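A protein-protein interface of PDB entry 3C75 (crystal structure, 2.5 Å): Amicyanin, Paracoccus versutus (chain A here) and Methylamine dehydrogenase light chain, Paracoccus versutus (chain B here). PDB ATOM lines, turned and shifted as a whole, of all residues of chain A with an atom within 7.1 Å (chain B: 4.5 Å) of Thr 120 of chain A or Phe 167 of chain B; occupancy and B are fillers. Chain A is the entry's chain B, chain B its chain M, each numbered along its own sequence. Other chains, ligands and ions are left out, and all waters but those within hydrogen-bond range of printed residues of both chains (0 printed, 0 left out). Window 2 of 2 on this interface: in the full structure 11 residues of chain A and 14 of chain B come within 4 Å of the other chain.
The backbone carbonyl oxygen (O) of Gly 168 of chain B lies within hydrogen-bond range of the guanidinium group (NH2) of Arg 95 of chain A, at 3.4 Å.
The side-chain hydroxyl (OG1) of Thr 111 of chain B sits at hydrogen-bond distance from the guanidinium group (NE) of Arg 95 of chain A, 3.4 Å away.
The backbone carbonyl oxygen (O) of Phe 167 of chain B lies within hydrogen-bond range of the backbone NH (N) of Ala 112 of chain B (3.5 Å).
N of Thr 111 of chain B is in hydrogen-bond range of O of Phe 167 of chain B, at 3.1 Å.
The side-chain amide oxygen (OD1) of Asn 81 of chain A sits at hydrogen-bond distance from the backbone NH (N) of Thr 120 of chain A, at 2.9 Å.
Among the printed residues, merely in contact across the chains: Met 98 of chain A with Thr 111 of chain B (3.3 Å), Pro 121 of chain A with Ala 112 of chain B (3.5 Å), Pro 121 of chain A with Trp 165 of chain B (3.6 Å), Thr 120 of chain A with Ala 112 of chain B (3.6 Å) and Thr 120 of chain A with Phe 167 of chain B (3.8 Å).
Printed residues of chain B within 4 Å of Arg 95 of chain A: Thr 111 (3.4 Å) and Gly 168 (3.4 Å).
Of the printed residues of chain B, Met 98 of chain A touches Thr 111 (3.3 Å).
Of chain B, only Ala 112 and Phe 167 come within 4 Å of Thr 120 of chain A.
Of the printed residues of chain A, Thr 111 of chain B touches Arg 95 and Met 98.
Of the printed residues of chain A, Ala 112 of chain B touches Thr 120 (3.6 Å) and Pro 121 (3.5 Å).
Of the printed residues of chain A, Trp 165 of chain B touches Pro 121.
Phe 167 of chain B touches just one residue of chain A: Thr 120.
Of the 17 printed residues of chain A, 4 touch a printed residue of chain B.
Hydrophobic or aromatic side chains of chain A that line the printed part of chain B: Met 98 and Pro 121.
Hydrophobic or aromatic side chains of chain B that line the printed part of chain A: Ala 112, Trp 165 and Phe 167.
Among the printed residues, 7 pairs touch across the chains.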
ATOM      1  N   TYR A  57      -3.919   1.243  -8.107  1.00  0.00           N
ATOM      2  CA  TYR A  57      -3.628   2.674  -8.198  1.00  0.00           C
ATOM      3  C   TYR A  57      -3.771   2.848  -9.712  1.00  0.00           C
ATOM      4  O   TYR A  57      -2.944   2.366 -10.471  1.00  0.00           O
ATOM      5  CB  TYR A  57      -2.183   2.975  -7.794  1.00  0.00           C
ATOM      6  CG  TYR A  57      -1.881   2.760  -6.327  1.00  0.00           C
ATOM      7  CD1 TYR A  57      -2.219   3.729  -5.367  1.00  0.00           C
ATOM      8  CD2 TYR A  57      -1.294   1.573  -5.886  1.00  0.00           C
ATOM      9  CE1 TYR A  57      -1.983   3.514  -4.015  1.00  0.00           C
ATOM     10  CE2 TYR A  57      -1.055   1.345  -4.526  1.00  0.00           C
ATOM     11  CZ  TYR A  57      -1.408   2.315  -3.603  1.00  0.00           C
ATOM     12  OH  TYR A  57      -1.234   2.057  -2.270  1.00  0.00           O
ATOM     13  N   HIS A  80      -7.888   1.910   1.546  1.00  0.00           N
ATOM     14  CA  HIS A  80      -6.578   1.867   0.899  1.00  0.00           C
ATOM     15  C   HIS A  80      -5.723   3.030   1.391  1.00  0.00           C
ATOM     16  O   HIS A  80      -6.231   4.012   1.929  1.00  0.00           O
ATOM     17  CB  HIS A  80      -6.728   2.015  -0.598  1.00  0.00           C
ATOM     18  CG  HIS A  80      -7.443   0.888  -1.274  1.00  0.00           C
ATOM     19  ND1 HIS A  80      -6.935  -0.391  -1.329  1.00  0.00           N
ATOM     20  CD2 HIS A  80      -8.556   0.881  -2.046  1.00  0.00           C
ATOM     21  CE1 HIS A  80      -7.693  -1.133  -2.116  1.00  0.00           C
ATOM     22  NE2 HIS A  80      -8.682  -0.385  -2.564  1.00  0.00           N
ATOM     23  N   ASN A  81      -4.421   2.936   1.182  1.00  0.00           N
ATOM     24  CA  ASN A  81      -3.526   3.996   1.623  1.00  0.00           C
ATOM     25  C   ASN A  81      -2.202   3.954   0.848  1.00  0.00           C
ATOM     26  O   ASN A  81      -2.006   3.115  -0.035  1.00  0.00           O
ATOM     27  CB  ASN A  81      -3.211   3.811   3.100  1.00  0.00           C
ATOM     28  CG  ASN A  81      -2.145   2.770   3.330  1.00  0.00           C
ATOM     29  OD1 ASN A  81      -2.034   1.793   2.587  1.00  0.00           O
ATOM     30  ND2 ASN A  81      -1.347   2.971   4.374  1.00  0.00           N
ATOM     31  N   VAL A  82      -1.298   4.870   1.187  1.00  0.00           N
ATOM     32  CA  VAL A  82       0.003   4.898   0.567  1.00  0.00           C
ATOM     33  C   VAL A  82       0.988   4.561   1.668  1.00  0.00           C
ATOM     34  O   VAL A  82       0.861   5.049   2.781  1.00  0.00           O
ATOM     35  CB  VAL A  82       0.328   6.285  -0.006  1.00  0.00           C
ATOM     36  CG1 VAL A  82       1.814   6.348  -0.502  1.00  0.00           C
ATOM     37  CG2 VAL A  82      -0.628   6.593  -1.120  1.00  0.00           C
ATOM     38  N   ALA A  83       1.960   3.721   1.342  1.00  0.00           N
ATOM     39  CA  ALA A  83       2.968   3.287   2.291  1.00  0.00           C
ATOM     40  C   ALA A  83       4.330   3.081   1.626  1.00  0.00           C
ATOM     41  O   ALA A  83       4.430   2.800   0.432  1.00  0.00           O
ATOM     42  CB  ALA A  83       2.514   1.993   2.952  1.00  0.00           C
ATOM     43  N   PHE A  84       5.390   3.220   2.401  1.00  0.00           N
ATOM     44  CA  PHE A  84       6.736   3.005   1.859  1.00  0.00           C
ATOM     45  C   PHE A  84       7.497   2.108   2.855  1.00  0.00           C
ATOM     46  O   PHE A  84       7.235   2.152   4.064  1.00  0.00           O
ATOM     47  CB  PHE A  84       7.502   4.341   1.706  1.00  0.00           C
ATOM     48  CG  PHE A  84       6.800   5.371   0.864  1.00  0.00           C
ATOM     49  CD1 PHE A  84       7.066   5.473  -0.498  1.00  0.00           C
ATOM     50  CD2 PHE A  84       5.878   6.245   1.433  1.00  0.00           C
ATOM     51  CE1 PHE A  84       6.420   6.434  -1.301  1.00  0.00           C
ATOM     52  CE2 PHE A  84       5.226   7.199   0.666  1.00  0.00           C
ATOM     53  CZ  PHE A  84       5.495   7.300  -0.719  1.00  0.00           C
ATOM     54  N   PHE A  94       7.461   4.545   6.206  1.00  0.00           N
ATOM     55  CA  PHE A  94       6.336   5.471   6.348  1.00  0.00           C
ATOM     56  C   PHE A  94       4.984   4.873   5.923  1.00  0.00           C
ATOM     57  O   PHE A  94       4.888   4.134   4.942  1.00  0.00           O
ATOM     58  CB  PHE A  94       6.613   6.769   5.582  1.00  0.00           C
ATOM     59  CG  PHE A  94       5.459   7.727   5.604  1.00  0.00           C
ATOM     60  CD1 PHE A  94       4.369   7.553   4.738  1.00  0.00           C
ATOM     61  CD2 PHE A  94       5.428   8.764   6.519  1.00  0.00           C
ATOM     62  CE1 PHE A  94       3.282   8.388   4.790  1.00  0.00           C
ATOM     63  CE2 PHE A  94       4.331   9.609   6.579  1.00  0.00           C
ATOM     64  CZ  PHE A  94       3.255   9.417   5.710  1.00  0.00           C
ATOM     65  N   ARG A  95       3.937   5.210   6.671  1.00  0.00           N
ATOM     66  CA  ARG A  95       2.602   4.669   6.410  1.00  0.00           C
ATOM     67  C   ARG A  95       1.498   5.729   6.498  1.00  0.00           C
ATOM     68  O   ARG A  95       1.135   6.187   7.574  1.00  0.00           O
ATOM     69  CB  ARG A  95       2.305   3.546   7.405  1.00  0.00           C
ATOM     70  CG  ARG A  95       1.039   2.791   7.083  1.00  0.00           C
ATOM     71  CD  ARG A  95       0.533   1.997   8.274  1.00  0.00           C
ATOM     72  NE  ARG A  95      -0.019   2.834   9.343  1.00  0.00           N
ATOM     73  CZ  ARG A  95       0.649   3.202  10.445  1.00  0.00           C
ATOM     74  NH1 ARG A  95       1.915   2.811  10.648  1.00  0.00           N
ATOM     75  NH2 ARG A  95       0.049   3.966  11.354  1.00  0.00           N
ATOM     76  N   GLY A  96       0.954   6.116   5.356  1.00  0.00           N
ATOM     77  CA  GLY A  96      -0.079   7.124   5.378  1.00  0.00           C
ATOM     78  C   GLY A  96      -1.323   6.591   6.037  1.00  0.00           C
ATOM     79  O   GLY A  96      -1.435   5.392   6.294  1.00  0.00           O
ATOM     80  N   MET A  98      -5.366   5.618   6.295  1.00  0.00           N
ATOM     81  CA  MET A  98      -6.257   4.950   5.346  1.00  0.00           C
ATOM     82  C   MET A  98      -7.274   5.919   4.777  1.00  0.00           C
ATOM     83  O   MET A  98      -7.568   6.939   5.393  1.00  0.00           O
ATOM     84  CB  MET A  98      -6.997   3.788   6.025  1.00  0.00           C
ATOM     85  CG  MET A  98      -6.095   2.696   6.544  1.00  0.00           C
ATOM     86  SD  MET A  98      -5.153   1.883   5.257  1.00  0.00           S
ATOM     87  CE  MET A  98      -6.352   0.923   4.498  1.00  0.00           C
ATOM     88  N   PHE A 118       3.373   1.189  -1.792  1.00  0.00           N
ATOM     89  CA  PHE A 118       2.412   0.093  -1.845  1.00  0.00           C
ATOM     90  C   PHE A 118       1.278   0.342  -0.896  1.00  0.00           C
ATOM     91  O   PHE A 118       1.265   1.340  -0.195  1.00  0.00           O
ATOM     92  CB  PHE A 118       3.074  -1.249  -1.464  1.00  0.00           C
ATOM     93  CG  PHE A 118       3.674  -1.278  -0.065  1.00  0.00           C
ATOM     94  CD1 PHE A 118       4.890  -0.620   0.216  1.00  0.00           C
ATOM     95  CD2 PHE A 118       3.002  -1.904   0.984  1.00  0.00           C
ATOM     96  CE1 PHE A 118       5.413  -0.577   1.519  1.00  0.00           C
ATOM     97  CE2 PHE A 118       3.514  -1.870   2.291  1.00  0.00           C
ATOM     98  CZ  PHE A 118       4.711  -1.209   2.561  1.00  0.00           C
ATOM     99  N   CYS A 119       0.318  -0.570  -0.875  1.00  0.00           N
ATOM    100  CA  CYS A 119      -0.806  -0.431   0.029  1.00  0.00           C
ATOM    101  C   CYS A 119      -0.504  -1.299   1.247  1.00  0.00           C
ATOM    102  O   CYS A 119      -0.115  -2.468   1.126  1.00  0.00           O
ATOM    103  CB  CYS A 119      -2.121  -0.862  -0.628  1.00  0.00           C
ATOM    104  SG  CYS A 119      -3.482  -0.346   0.412  1.00  0.00           S
ATOM    105  N   THR A 120      -0.672  -0.716   2.429  1.00  0.00           N
ATOM    106  CA  THR A 120      -0.358  -1.430   3.656  1.00  0.00           C
ATOM    107  C   THR A 120      -0.910  -2.842   3.771  1.00  0.00           C
ATOM    108  O   THR A 120      -0.129  -3.793   3.847  1.00  0.00           O
ATOM    109  CB  THR A 120      -0.766  -0.634   4.896  1.00  0.00           C
ATOM    110  OG1 THR A 120       0.159   0.462   5.104  1.00  0.00           O
ATOM    111  CG2 THR A 120      -0.771  -1.564   6.101  1.00  0.00           C
ATOM    112  N   PRO A 121      -2.256  -3.000   3.784  1.00  0.00           N
ATOM    113  CA  PRO A 121      -2.897  -4.314   3.883  1.00  0.00           C
ATOM    114  C   PRO A 121      -2.887  -5.045   2.543  1.00  0.00           C
ATOM    115  O   PRO A 121      -2.986  -6.268   2.483  1.00  0.00           O
ATOM    116  CB  PRO A 121      -4.290  -3.952   4.319  1.00  0.00           C
ATOM    117  CG  PRO A 121      -4.539  -2.725   3.525  1.00  0.00           C
ATOM    118  CD  PRO A 121      -3.287  -1.941   3.739  1.00  0.00           C
ATOM    119  N   HIS A 122      -2.730  -4.285   1.466  1.00  0.00           N
ATOM    120  CA  HIS A 122      -2.719  -4.831   0.117  1.00  0.00           C
ATOM    121  C   HIS A 122      -1.322  -4.668  -0.571  1.00  0.00           C
ATOM    122  O   HIS A 122      -1.127  -3.774  -1.405  1.00  0.00           O
ATOM    123  CB  HIS A 122      -3.838  -4.126  -0.670  1.00  0.00           C
ATOM    124  CG  HIS A 122      -5.172  -4.142   0.025  1.00  0.00           C
ATOM    125  ND1 HIS A 122      -6.028  -3.061   0.028  1.00  0.00           N
ATOM    126  CD2 HIS A 122      -5.808  -5.118   0.719  1.00  0.00           C
ATOM    127  CE1 HIS A 122      -7.130  -3.366   0.690  1.00  0.00           C
ATOM    128  NE2 HIS A 122      -7.023  -4.609   1.118  1.00  0.00           N
ATOM    129  N   PRO A 123      -0.345  -5.546  -0.233  1.00  0.00           N
ATOM    130  CA  PRO A 123       1.031  -5.565  -0.757  1.00  0.00           C
ATOM    131  C   PRO A 123       1.089  -5.761  -2.276  1.00  0.00           C
ATOM    132  O   PRO A 123       2.095  -5.444  -2.943  1.00  0.00           O
ATOM    133  CB  PRO A 123       1.672  -6.754  -0.035  1.00  0.00           C
ATOM    134  CG  PRO A 123       0.835  -6.961   1.143  1.00  0.00           C
ATOM    135  CD  PRO A 123      -0.556  -6.704   0.640  1.00  0.00           C
ATOM    136  N   MET A 125      -0.527  -4.135  -4.247  1.00  0.00           N
ATOM    137  CA  MET A 125      -0.831  -2.850  -4.867  1.00  0.00           C
ATOM    138  C   MET A 125       0.407  -1.936  -4.805  1.00  0.00           C
ATOM    139  O   MET A 125       0.817  -1.509  -3.730  1.00  0.00           O
ATOM    140  CB  MET A 125      -1.995  -2.189  -4.140  1.00  0.00           C
ATOM    141  CG  MET A 125      -3.326  -2.816  -4.453  1.00  0.00           C
ATOM    142  SD  MET A 125      -4.626  -2.113  -3.412  1.00  0.00           S
ATOM    143  CE  MET A 125      -4.667  -0.341  -4.000  1.00  0.00           C
ATOM    144  N   ALA B 110      -4.510  -1.716  15.040  1.00  0.00           N
ATOM    145  CA  ALA B 110      -4.021  -1.854  13.690  1.00  0.00           C
ATOM    146  C   ALA B 110      -4.828  -0.807  12.909  1.00  0.00           C
ATOM    147  O   ALA B 110      -5.874  -0.364  13.387  1.00  0.00           O
ATOM    148  CB  ALA B 110      -4.302  -3.269  13.164  1.00  0.00           C
ATOM    149  N   THR B 111      -4.343  -0.404  11.732  1.00  0.00           N
ATOM    150  CA  THR B 111      -5.033   0.587  10.899  1.00  0.00           C
ATOM    151  C   THR B 111      -5.551  -0.100   9.645  1.00  0.00           C
ATOM    152  O   THR B 111      -6.404   0.436   8.943  1.00  0.00           O
ATOM    153  CB  THR B 111      -4.064   1.726  10.482  1.00  0.00           C
ATOM    154  OG1 THR B 111      -2.990   1.206   9.684  1.00  0.00           O
ATOM    155  CG2 THR B 111      -3.476   2.332  11.691  1.00  0.00           C
ATOM    156  N   ALA B 112      -5.031  -1.301   9.385  1.00  0.00           N
ATOM    157  CA  ALA B 112      -5.378  -2.070   8.190  1.00  0.00           C
ATOM    158  C   ALA B 112      -6.028  -3.406   8.505  1.00  0.00           C
ATOM    159  O   ALA B 112      -5.929  -3.891   9.612  1.00  0.00           O
ATOM    160  CB  ALA B 112      -4.112  -2.296   7.359  1.00  0.00           C
ATOM    161  N   ILE B 164      -3.195 -12.315  10.302  1.00  0.00           N
ATOM    162  CA  ILE B 164      -3.111 -11.478  11.500  1.00  0.00           C
ATOM    163  C   ILE B 164      -2.987 -10.038  11.018  1.00  0.00           C
ATOM    164  O   ILE B 164      -1.912  -9.581  10.621  1.00  0.00           O
ATOM    165  CB  ILE B 164      -1.909 -11.854  12.438  1.00  0.00           C
ATOM    166  CG1 ILE B 164      -2.105 -13.262  13.011  1.00  0.00           C
ATOM    167  CG2 ILE B 164      -1.780 -10.836  13.542  1.00  0.00           C
ATOM    168  CD1 ILE B 164      -3.520 -13.518  13.589  1.00  0.00           C
ATOM    169  N   TRP B 165      -4.128  -9.352  11.067  1.00  0.00           N
ATOM    170  CA  TRP B 165      -4.280  -7.973  10.628  1.00  0.00           C
ATOM    171  C   TRP B 165      -3.839  -6.947  11.685  1.00  0.00           C
ATOM    172  O   TRP B 165      -4.636  -6.149  12.188  1.00  0.00           O
ATOM    173  CB  TRP B 165      -5.755  -7.765  10.182  1.00  0.00           C
ATOM    174  CG  TRP B 165      -6.090  -8.459   8.838  1.00  0.00           C
ATOM    175  CD1 TRP B 165      -7.165  -9.322   8.527  1.00  0.00           C
ATOM    176  CD2 TRP B 165      -5.338  -8.327   7.622  1.00  0.00           C
ATOM    177  NE1 TRP B 165      -7.075  -9.694   7.211  1.00  0.00           N
ATOM    178  CE2 TRP B 165      -5.987  -9.107   6.633  1.00  0.00           C
ATOM    179  CE3 TRP B 165      -4.183  -7.618   7.269  1.00  0.00           C
ATOM    180  CZ2 TRP B 165      -5.520  -9.192   5.328  1.00  0.00           C
ATOM    181  CZ3 TRP B 165      -3.715  -7.695   5.975  1.00  0.00           C
ATOM    182  CH2 TRP B 165      -4.383  -8.479   5.011  1.00  0.00           C
ATOM    183  N   CYS B 166      -2.549  -6.963  12.009  1.00  0.00           N
ATOM    184  CA  CYS B 166      -1.991  -6.054  13.006  1.00  0.00           C
ATOM    185  C   CYS B 166      -1.189  -4.925  12.405  1.00  0.00           C
ATOM    186  O   CYS B 166      -0.644  -4.080  13.116  1.00  0.00           O
ATOM    187  CB  CYS B 166      -1.118  -6.843  13.957  1.00  0.00           C
ATOM    188  SG  CYS B 166      -2.183  -7.718  15.118  1.00  0.00           S
ATOM    189  N   PHE B 167      -1.119  -4.905  11.083  1.00  0.00           N
ATOM    190  CA  PHE B 167      -0.341  -3.893  10.382  1.00  0.00           C
ATOM    191  C   PHE B 167      -0.720  -2.446  10.750  1.00  0.00           C
ATOM    192  O   PHE B 167      -1.902  -2.061  10.738  1.00  0.00           O
ATOM    193  CB  PHE B 167      -0.461  -4.151   8.868  1.00  0.00           C
ATOM    194  CG  PHE B 167      -0.014  -5.545   8.451  1.00  0.00           C
ATOM    195  CD1 PHE B 167       1.313  -5.971   8.669  1.00  0.00           C
ATOM    196  CD2 PHE B 167      -0.927  -6.455   7.915  1.00  0.00           C
ATOM    197  CE1 PHE B 167       1.703  -7.295   8.366  1.00  0.00           C
ATOM    198  CE2 PHE B 167      -0.542  -7.766   7.614  1.00  0.00           C
ATOM    199  CZ  PHE B 167       0.767  -8.189   7.843  1.00  0.00           C
ATOM    200  N   GLY B 168       0.286  -1.649  11.093  1.00  0.00           N
ATOM    201  CA  GLY B 168       0.015  -0.268  11.433  1.00  0.00           C
ATOM    202  C   GLY B 168      -0.288   0.032  12.899  1.00  0.00           C
ATOM    203  O   GLY B 168      -0.566   1.190  13.253  1.00  0.00           O
ATOM    204  N   ALA B 169      -0.267  -0.993  13.746  1.00  0.00           N
ATOM    205  CA  ALA B 169      -0.514  -0.795  15.173  1.00  0.00           C
ATOM    206  C   ALA B 169       0.724  -0.138  15.799  1.00  0.00           C
ATOM    207  O   ALA B 169       1.851  -0.388  15.369  1.00  0.00           O
ATOM    208  CB  ALA B 169      -0.798  -2.137  15.867  1.00  0.00           C
ATOM    209  N   MET B 174       2.386  -7.181  16.704  1.00  0.00           N
ATOM    210  CA  MET B 174       1.919  -8.098  15.687  1.00  0.00           C
ATOM    211  C   MET B 174       1.187  -9.311  16.242  1.00  0.00           C
ATOM    212  O   MET B 174       0.834 -10.196  15.478  1.00  0.00           O
ATOM    213  CB  MET B 174       3.094  -8.591  14.826  1.00  0.00           C
ATOM    214  CG  MET B 174       3.449  -7.687  13.635  1.00  0.00           C
ATOM    215  SD  MET B 174       2.021  -7.096  12.696  1.00  0.00           S
ATOM    216  CE  MET B 174       1.343  -8.619  12.013  1.00  0.00           C
